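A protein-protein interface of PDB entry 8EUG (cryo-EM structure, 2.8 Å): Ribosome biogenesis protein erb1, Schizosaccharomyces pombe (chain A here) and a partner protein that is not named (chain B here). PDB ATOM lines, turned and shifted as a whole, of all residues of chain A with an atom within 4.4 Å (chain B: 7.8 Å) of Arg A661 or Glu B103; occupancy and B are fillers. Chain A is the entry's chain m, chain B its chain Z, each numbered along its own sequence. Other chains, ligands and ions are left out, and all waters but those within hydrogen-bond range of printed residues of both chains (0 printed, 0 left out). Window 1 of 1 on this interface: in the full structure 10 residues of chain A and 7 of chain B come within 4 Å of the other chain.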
ATOM      1  N   ARG A 385     -37.582  16.309 -28.019  1.00  0.00           N
ATOM      2  CA  ARG A 385     -36.442  17.135 -28.392  1.00  0.00           C
ATOM      3  C   ARG A 385     -35.753  16.574 -29.629  1.00  0.00           C
ATOM      4  O   ARG A 385     -35.578  15.360 -29.767  1.00  0.00           O
ATOM      5  CB  ARG A 385     -35.447  17.223 -27.235  1.00  0.00           C
ATOM      6  CG  ARG A 385     -36.043  17.732 -25.935  1.00  0.00           C
ATOM      7  CD  ARG A 385     -34.987  17.823 -24.846  1.00  0.00           C
ATOM      8  NE  ARG A 385     -34.199  16.600 -24.749  1.00  0.00           N
ATOM      9  CZ  ARG A 385     -33.264  16.382 -23.835  1.00  0.00           C
ATOM     10  NH1 ARG A 385     -32.971  17.289 -22.918  1.00  0.00           N
ATOM     11  NH2 ARG A 385     -32.607  15.226 -23.841  1.00  0.00           N
ATOM     12  N   SER A 618     -18.308  22.385 -25.446  1.00  0.00           N
ATOM     13  CA  SER A 618     -19.550  21.775 -25.915  1.00  0.00           C
ATOM     14  C   SER A 618     -19.403  21.162 -27.305  1.00  0.00           C
ATOM     15  O   SER A 618     -19.577  19.952 -27.480  1.00  0.00           O
ATOM     16  CB  SER A 618     -20.673  22.818 -25.914  1.00  0.00           C
ATOM     17  OG  SER A 618     -21.813  22.336 -26.604  1.00  0.00           O
ATOM     18  N   SER A 619     -19.085  21.986 -28.301  1.00  0.00           N
ATOM     19  CA  SER A 619     -18.999  21.529 -29.680  1.00  0.00           C
ATOM     20  C   SER A 619     -17.950  22.355 -30.408  1.00  0.00           C
ATOM     21  O   SER A 619     -17.510  23.402 -29.927  1.00  0.00           O
ATOM     22  CB  SER A 619     -20.356  21.626 -30.388  1.00  0.00           C
ATOM     23  OG  SER A 619     -21.327  20.820 -29.747  1.00  0.00           O
ATOM     24  N   TYR A 634     -20.076  25.179 -22.773  1.00  0.00           N
ATOM     25  CA  TYR A 634     -21.116  25.226 -21.755  1.00  0.00           C
ATOM     26  C   TYR A 634     -21.000  26.460 -20.870  1.00  0.00           C
ATOM     27  O   TYR A 634     -21.940  26.762 -20.126  1.00  0.00           O
ATOM     28  CB  TYR A 634     -21.049  23.956 -20.906  1.00  0.00           C
ATOM     29  CG  TYR A 634     -21.368  22.699 -21.685  1.00  0.00           C
ATOM     30  CD1 TYR A 634     -22.310  22.708 -22.703  1.00  0.00           C
ATOM     31  CD2 TYR A 634     -20.689  21.516 -21.434  1.00  0.00           C
ATOM     32  CE1 TYR A 634     -22.596  21.563 -23.424  1.00  0.00           C
ATOM     33  CE2 TYR A 634     -20.959  20.367 -22.155  1.00  0.00           C
ATOM     34  CZ  TYR A 634     -21.914  20.397 -23.149  1.00  0.00           C
ATOM     35  OH  TYR A 634     -22.188  19.255 -23.865  1.00  0.00           O
ATOM     36  N   ALA A 659     -26.029  27.981 -21.376  1.00  0.00           N
ATOM     37  CA  ALA A 659     -24.957  27.172 -21.938  1.00  0.00           C
ATOM     38  C   ALA A 659     -25.106  27.064 -23.450  1.00  0.00           C
ATOM     39  O   ALA A 659     -26.189  26.765 -23.961  1.00  0.00           O
ATOM     40  CB  ALA A 659     -24.956  25.782 -21.305  1.00  0.00           C
ATOM     41  N   LEU A 660     -24.012  27.311 -24.163  1.00  0.00           N
ATOM     42  CA  LEU A 660     -24.032  27.271 -25.618  1.00  0.00           C
ATOM     43  C   LEU A 660     -23.891  25.825 -26.077  1.00  0.00           C
ATOM     44  O   LEU A 660     -22.996  25.107 -25.620  1.00  0.00           O
ATOM     45  CB  LEU A 660     -22.911  28.138 -26.190  1.00  0.00           C
ATOM     46  CG  LEU A 660     -22.873  28.394 -27.699  1.00  0.00           C
ATOM     47  CD1 LEU A 660     -22.161  29.708 -27.969  1.00  0.00           C
ATOM     48  CD2 LEU A 660     -22.219  27.266 -28.466  1.00  0.00           C
ATOM     49  N   ARG A 661     -24.772  25.402 -26.980  1.00  0.00           N
ATOM     50  CA  ARG A 661     -24.842  23.994 -27.351  1.00  0.00           C
ATOM     51  C   ARG A 661     -24.031  23.671 -28.602  1.00  0.00           C
ATOM     52  O   ARG A 661     -23.174  22.782 -28.570  1.00  0.00           O
ATOM     53  CB  ARG A 661     -26.304  23.580 -27.547  1.00  0.00           C
ATOM     54  CG  ARG A 661     -27.139  23.677 -26.283  1.00  0.00           C
ATOM     55  CD  ARG A 661     -26.435  23.033 -25.099  1.00  0.00           C
ATOM     56  NE  ARG A 661     -26.274  21.593 -25.265  1.00  0.00           N
ATOM     57  CZ  ARG A 661     -27.068  20.685 -24.715  1.00  0.00           C
ATOM     58  NH1 ARG A 661     -28.093  21.033 -23.954  1.00  0.00           N
ATOM     59  NH2 ARG A 661     -26.829  19.396 -24.932  1.00  0.00           N
ATOM     60  N   ASP A 662     -24.284  24.369 -29.707  1.00  0.00           N
ATOM     61  CA  ASP A 662     -23.702  24.007 -30.990  1.00  0.00           C
ATOM     62  C   ASP A 662     -23.174  25.253 -31.688  1.00  0.00           C
ATOM     63  O   ASP A 662     -23.737  26.344 -31.563  1.00  0.00           O
ATOM     64  CB  ASP A 662     -24.751  23.284 -31.867  1.00  0.00           C
ATOM     65  CG  ASP A 662     -24.313  23.105 -33.315  1.00  0.00           C
ATOM     66  OD1 ASP A 662     -23.113  23.254 -33.624  1.00  0.00           O
ATOM     67  OD2 ASP A 662     -25.188  22.809 -34.155  1.00  0.00           O
ATOM     68  N   GLY A 675     -25.875  28.099 -31.390  1.00  0.00           N
ATOM     69  CA  GLY A 675     -27.150  27.773 -30.776  1.00  0.00           C
ATOM     70  C   GLY A 675     -26.955  27.393 -29.318  1.00  0.00           C
ATOM     71  O   GLY A 675     -26.125  26.540 -28.996  1.00  0.00           O
ATOM     72  N   SER A 676     -27.728  28.037 -28.449  1.00  0.00           N
ATOM     73  CA  SER A 676     -27.622  27.845 -27.010  1.00  0.00           C
ATOM     74  C   SER A 676     -28.966  27.423 -26.432  1.00  0.00           C
ATOM     75  O   SER A 676     -29.989  27.393 -27.122  1.00  0.00           O
ATOM     76  CB  SER A 676     -27.125  29.121 -26.320  1.00  0.00           C
ATOM     77  OG  SER A 676     -27.269  29.029 -24.913  1.00  0.00           O
ATOM     78  N   ASP A 677     -28.953  27.104 -25.138  1.00  0.00           N
ATOM     79  CA  ASP A 677     -30.148  26.637 -24.448  1.00  0.00           C
ATOM     80  C   ASP A 677     -31.108  27.759 -24.080  1.00  0.00           C
ATOM     81  O   ASP A 677     -32.241  27.473 -23.678  1.00  0.00           O
ATOM     82  CB  ASP A 677     -29.757  25.862 -23.187  1.00  0.00           C
ATOM     83  CG  ASP A 677     -29.300  24.451 -23.492  1.00  0.00           C
ATOM     84  OD1 ASP A 677     -29.797  23.864 -24.476  1.00  0.00           O
ATOM     85  OD2 ASP A 677     -28.443  23.926 -22.751  1.00  0.00           O
ATOM     86  N   VAL A 713     -34.095  23.527 -21.892  1.00  0.00           N
ATOM     87  CA  VAL A 713     -33.313  23.145 -23.063  1.00  0.00           C
ATOM     88  C   VAL A 713     -33.794  23.979 -24.241  1.00  0.00           C
ATOM     89  O   VAL A 713     -35.000  24.045 -24.507  1.00  0.00           O
ATOM     90  CB  VAL A 713     -33.438  21.642 -23.377  1.00  0.00           C
ATOM     91  CG1 VAL A 713     -32.666  21.295 -24.641  1.00  0.00           C
ATOM     92  CG2 VAL A 713     -32.946  20.808 -22.203  1.00  0.00           C
ATOM     93  N   VAL A 715     -31.982  25.815 -28.110  1.00  0.00           N
ATOM     94  CA  VAL A 715     -31.458  25.454 -29.424  1.00  0.00           C
ATOM     95  C   VAL A 715     -30.402  24.370 -29.231  1.00  0.00           C
ATOM     96  O   VAL A 715     -29.319  24.631 -28.701  1.00  0.00           O
ATOM     97  CB  VAL A 715     -30.880  26.671 -30.152  1.00  0.00           C
ATOM     98  CG1 VAL A 715     -30.509  26.307 -31.576  1.00  0.00           C
ATOM     99  CG2 VAL A 715     -31.876  27.818 -30.127  1.00  0.00           C
ATOM    100  N   LEU A 716     -30.715  23.149 -29.662  1.00  0.00           N
ATOM    101  CA  LEU A 716     -29.823  22.016 -29.460  1.00  0.00           C
ATOM    102  C   LEU A 716     -28.825  21.845 -30.600  1.00  0.00           C
ATOM    103  O   LEU A 716     -27.639  21.606 -30.350  1.00  0.00           O
ATOM    104  CB  LEU A 716     -30.641  20.734 -29.289  1.00  0.00           C
ATOM    105  CG  LEU A 716     -29.945  19.568 -28.585  1.00  0.00           C
ATOM    106  CD1 LEU A 716     -29.209  20.060 -27.352  1.00  0.00           C
ATOM    107  CD2 LEU A 716     -30.951  18.495 -28.212  1.00  0.00           C
ATOM    108  N   THR B  97     -30.903  13.043 -12.227  1.00  0.00           N
ATOM    109  CA  THR B  97     -30.809  11.783 -12.959  1.00  0.00           C
ATOM    110  C   THR B  97     -29.530  11.834 -13.786  1.00  0.00           C
ATOM    111  O   THR B  97     -28.778  12.813 -13.740  1.00  0.00           O
ATOM    112  CB  THR B  97     -32.040  11.544 -13.839  1.00  0.00           C
ATOM    113  OG1 THR B  97     -31.927  10.275 -14.497  1.00  0.00           O
ATOM    114  CG2 THR B  97     -32.176  12.645 -14.880  1.00  0.00           C
ATOM    115  N   ALA B  98     -29.274  10.752 -14.527  1.00  0.00           N
ATOM    116  CA  ALA B  98     -28.152  10.753 -15.461  1.00  0.00           C
ATOM    117  C   ALA B  98     -28.356  11.790 -16.558  1.00  0.00           C
ATOM    118  O   ALA B  98     -27.412  12.485 -16.945  1.00  0.00           O
ATOM    119  CB  ALA B  98     -27.963   9.361 -16.062  1.00  0.00           C
ATOM    120  N   ASP B  99     -29.589  11.915 -17.059  1.00  0.00           N
ATOM    121  CA  ASP B  99     -29.888  12.905 -18.092  1.00  0.00           C
ATOM    122  C   ASP B  99     -29.550  14.314 -17.623  1.00  0.00           C
ATOM    123  O   ASP B  99     -29.153  15.167 -18.427  1.00  0.00           O
ATOM    124  CB  ASP B  99     -31.362  12.806 -18.493  1.00  0.00           C
ATOM    125  CG  ASP B  99     -31.662  13.489 -19.816  1.00  0.00           C
ATOM    126  OD1 ASP B  99     -30.716  13.729 -20.594  1.00  0.00           O
ATOM    127  OD2 ASP B  99     -32.849  13.773 -20.083  1.00  0.00           O
ATOM    128  N   THR B 100     -29.715  14.582 -16.326  1.00  0.00           N
ATOM    129  CA  THR B 100     -29.377  15.897 -15.791  1.00  0.00           C
ATOM    130  C   THR B 100     -27.875  16.154 -15.859  1.00  0.00           C
ATOM    131  O   THR B 100     -27.443  17.274 -16.153  1.00  0.00           O
ATOM    132  CB  THR B 100     -29.877  16.022 -14.353  1.00  0.00           C
ATOM    133  OG1 THR B 100     -31.295  15.812 -14.322  1.00  0.00           O
ATOM    134  CG2 THR B 100     -29.578  17.411 -13.813  1.00  0.00           C
ATOM    135  N   PHE B 101     -27.063  15.135 -15.575  1.00  0.00           N
ATOM    136  CA  PHE B 101     -25.615  15.324 -15.590  1.00  0.00           C
ATOM    137  C   PHE B 101     -25.090  15.534 -17.005  1.00  0.00           C
ATOM    138  O   PHE B 101     -24.225  16.390 -17.229  1.00  0.00           O
ATOM    139  CB  PHE B 101     -24.927  14.136 -14.925  1.00  0.00           C
ATOM    140  CG  PHE B 101     -24.850  14.249 -13.434  1.00  0.00           C
ATOM    141  CD1 PHE B 101     -25.861  13.744 -12.638  1.00  0.00           C
ATOM    142  CD2 PHE B 101     -23.775  14.876 -12.831  1.00  0.00           C
ATOM    143  CE1 PHE B 101     -25.795  13.857 -11.267  1.00  0.00           C
ATOM    144  CE2 PHE B 101     -23.703  14.990 -11.462  1.00  0.00           C
ATOM    145  CZ  PHE B 101     -24.714  14.481 -10.676  1.00  0.00           C
ATOM    146  N   LYS B 102     -25.591  14.760 -17.971  1.00  0.00           N
ATOM    147  CA  LYS B 102     -25.210  14.973 -19.367  1.00  0.00           C
ATOM    148  C   LYS B 102     -25.639  16.351 -19.852  1.00  0.00           C
ATOM    149  O   LYS B 102     -24.888  17.031 -20.559  1.00  0.00           O
ATOM    150  CB  LYS B 102     -25.780  13.880 -20.287  1.00  0.00           C
ATOM    151  CG  LYS B 102     -25.994  12.441 -19.754  1.00  0.00           C
ATOM    152  CD  LYS B 102     -24.958  11.962 -18.730  1.00  0.00           C
ATOM    153  CE  LYS B 102     -24.696  10.466 -18.887  1.00  0.00           C
ATOM    154  NZ  LYS B 102     -23.707   9.946 -17.898  1.00  0.00           N
ATOM    155  N   GLU B 103     -26.853  16.775 -19.499  1.00  0.00           N
ATOM    156  CA  GLU B 103     -27.336  18.100 -19.875  1.00  0.00           C
ATOM    157  C   GLU B 103     -26.800  19.156 -18.916  1.00  0.00           C
ATOM    158  O   GLU B 103     -27.333  19.315 -17.811  1.00  0.00           O
ATOM    159  CB  GLU B 103     -28.866  18.131 -19.892  1.00  0.00           C
ATOM    160  CG  GLU B 103     -29.494  17.617 -21.176  1.00  0.00           C
ATOM    161  CD  GLU B 103     -29.669  18.709 -22.211  1.00  0.00           C
ATOM    162  OE1 GLU B 103     -29.072  19.795 -22.041  1.00  0.00           O
ATOM    163  OE2 GLU B 103     -30.407  18.486 -23.193  1.00  0.00           O
ATOM    164  N   PRO B 104     -25.771  19.917 -19.304  1.00  0.00           N
ATOM    165  CA  PRO B 104     -25.148  20.838 -18.341  1.00  0.00           C
ATOM    166  C   PRO B 104     -26.076  21.942 -17.878  1.00  0.00           C
ATOM    167  O   PRO B 104     -25.964  22.385 -16.728  1.00  0.00           O
ATOM    168  CB  PRO B 104     -23.946  21.401 -19.113  1.00  0.00           C
ATOM    169  CG  PRO B 104     -23.812  20.525 -20.321  1.00  0.00           C
ATOM    170  CD  PRO B 104     -25.186  20.065 -20.643  1.00  0.00           C
ATOM    171  N   THR B 105     -26.980  22.410 -18.739  1.00  0.00           N
ATOM    172  CA  THR B 105     -27.940  23.422 -18.314  1.00  0.00           C
ATOM    173  C   THR B 105     -28.861  22.871 -17.233  1.00  0.00           C
ATOM    174  O   THR B 105     -29.225  23.586 -16.291  1.00  0.00           O
ATOM    175  CB  THR B 105     -28.745  23.920 -19.510  1.00  0.00           C
ATOM    176  OG1 THR B 105     -27.860  24.151 -20.614  1.00  0.00           O
ATOM    177  CG2 THR B 105     -29.438  25.222 -19.164  1.00  0.00           C
ATOM    178  N   GLN B 106     -29.250  21.600 -17.354  1.00  0.00           N
ATOM    179  CA  GLN B 106     -30.012  20.956 -16.291  1.00  0.00           C
ATOM    180  C   GLN B 106     -29.175  20.787 -15.029  1.00  0.00           C
ATOM    181  O   GLN B 106     -29.712  20.869 -13.918  1.00  0.00           O
ATOM    182  CB  GLN B 106     -30.537  19.602 -16.766  1.00  0.00           C
ATOM    183  CG  GLN B 106     -31.581  19.697 -17.865  1.00  0.00           C
ATOM    184  CD  GLN B 106     -32.069  18.337 -18.324  1.00  0.00           C
ATOM    185  OE1 GLN B 106     -31.580  17.303 -17.870  1.00  0.00           O
ATOM    186  NE2 GLN B 106     -33.038  18.334 -19.232  1.00  0.00           N
ATOM    187  N   ARG B 107     -27.870  20.542 -15.177  1.00  0.00           N
ATOM    188  CA  ARG B 107     -26.999  20.453 -14.009  1.00  0.00           C
ATOM    189  C   ARG B 107     -26.960  21.777 -13.258  1.00  0.00           C
ATOM    190  O   ARG B 107     -27.065  21.811 -12.026  1.00  0.00           O
ATOM    191  CB  ARG B 107     -25.588  20.037 -14.426  1.00  0.00           C
ATOM    192  CG  ARG B 107     -24.645  19.858 -13.245  1.00  0.00           C
ATOM    193  CD  ARG B 107     -23.230  19.492 -13.670  1.00  0.00           C
ATOM    194  NE  ARG B 107     -23.128  18.148 -14.223  1.00  0.00           N
ATOM    195  CZ  ARG B 107     -21.981  17.541 -14.493  1.00  0.00           C
ATOM    196  NH1 ARG B 107     -20.818  18.118 -14.238  1.00  0.00           N
ATOM    197  NH2 ARG B 107     -21.999  16.323 -15.027  1.00  0.00           N
ATOM    198  N   SER B 108     -26.802  22.884 -13.987  1.00  0.00           N
ATOM    199  CA  SER B 108     -26.820  24.198 -13.353  1.00  0.00           C
ATOM    200  C   SER B 108     -28.194  24.516 -12.781  1.00  0.00           C
ATOM    201  O   SER B 108     -28.301  25.098 -11.695  1.00  0.00           O
ATOM    202  CB  SER B 108     -26.394  25.270 -14.355  1.00  0.00           C
ATOM    203  OG  SER B 108     -25.045  25.090 -14.751  1.00  0.00           O
ATOM    204  N   ALA B 109     -29.258  24.153 -13.503  1.00  0.00           N
ATOM    205  CA  ALA B 109     -30.609  24.398 -13.006  1.00  0.00           C
ATOM    206  C   ALA B 109     -30.881  23.608 -11.734  1.00  0.00           C
ATOM    207  O   ALA B 109     -31.477  24.132 -10.785  1.00  0.00           O
ATOM    208  CB  ALA B 109     -31.636  24.049 -14.082  1.00  0.00           C
ATOM    209  N   ALA B 110     -30.457  22.343 -11.697  1.00  0.00           N
ATOM    210  CA  ALA B 110     -30.611  21.550 -10.483  1.00  0.00           C
ATOM    211  C   ALA B 110     -29.779  22.124  -9.345  1.00  0.00           C
ATOM    212  O   ALA B 110     -30.217  22.126  -8.188  1.00  0.00           O
ATOM    213  CB  ALA B 110     -30.226  20.096 -10.751  1.00  0.00           C
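The side-chain carboxylate of Asp A677 lies close to the side-chain hydroxyl of Thr B105 (2.2 Å). The guanidinium group (NH1) of Arg A385 is in salt-bridge range of the side-chain carboxylate (OE2) of Glu B103. The side-chain carboxylate (OE1) of Glu B103 lies within salt-bridge range of the guanidinium group (NH1) of Arg A661 (2.5 Å).
O of Ala A659 lies within hydrogen-bond range of N of Asp A677, 3.0 Å away. N of Arg A661 lies within hydrogen-bond range of O of Gly A675. OG of Ser B108 sits at hydrogen-bond distance from O of Pro B104, at 3.5 Å. The backbone carbonyl oxygen of Arg A661 lies within hydrogen-bond range of the side-chain hydroxyl of Ser A619 (2.9 Å). The backbone carbonyl oxygen (O) of Asp B99 sits close to the side-chain amide oxygen (OE1) of Gln B106 (3.3 Å). The guanidinium group (NH1) of Arg A661 is in salt-bridge range of the side-chain carboxylate (OD2) of Asp A677, 3.2 Å away.
Among the printed residues, merely in contact across the chains: Tyr A634 with Pro B104, Ala A659 with Thr B105, Val A713 with Glu B103, Arg A385 with Gln B106 and Val A713 with Gln B106.
Arg A661 touches just one residue of chain B: Glu B103. Of chain A, only Arg A385, Arg A661 and Val A713 come within 4 Å of Glu B103. Of the printed residues of chain A, Gln B106 touches Arg A385 (3.8 Å) and Val A713 (3.9 Å). Of the printed residues of chain A, Thr B105 touches Ala A659 (3.4 Å) and Asp A677 (2.2 Å). Thr B97 touches none of the printed residues of chain A. The nearest residue of chain B that does not touch Arg A661 is Pro B104 (4.5 Å). The nearest residue of chain A that does not touch Glu B103 is Asp A677 (4.2 Å). The nearest printed residue of chain A that does not touch Gln B106 is Asp A677 (5.9 Å).
Printed residues of chain A that touch a printed residue of chain B: Arg A385, Tyr A634, Ala A659, Arg A661, Asp A677 and Val A713. Of the 14 printed residues of chain B, 4 touch a printed residue of chain A. Among the printed residues, 8 pairs touch across the chains. Among the printed residues, Asp or Glu carboxylates within 4 Å of a Lys or Arg side-chain nitrogen of the other chain: Arg A385 with Glu B103 and Arg A661 with Glu B103.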
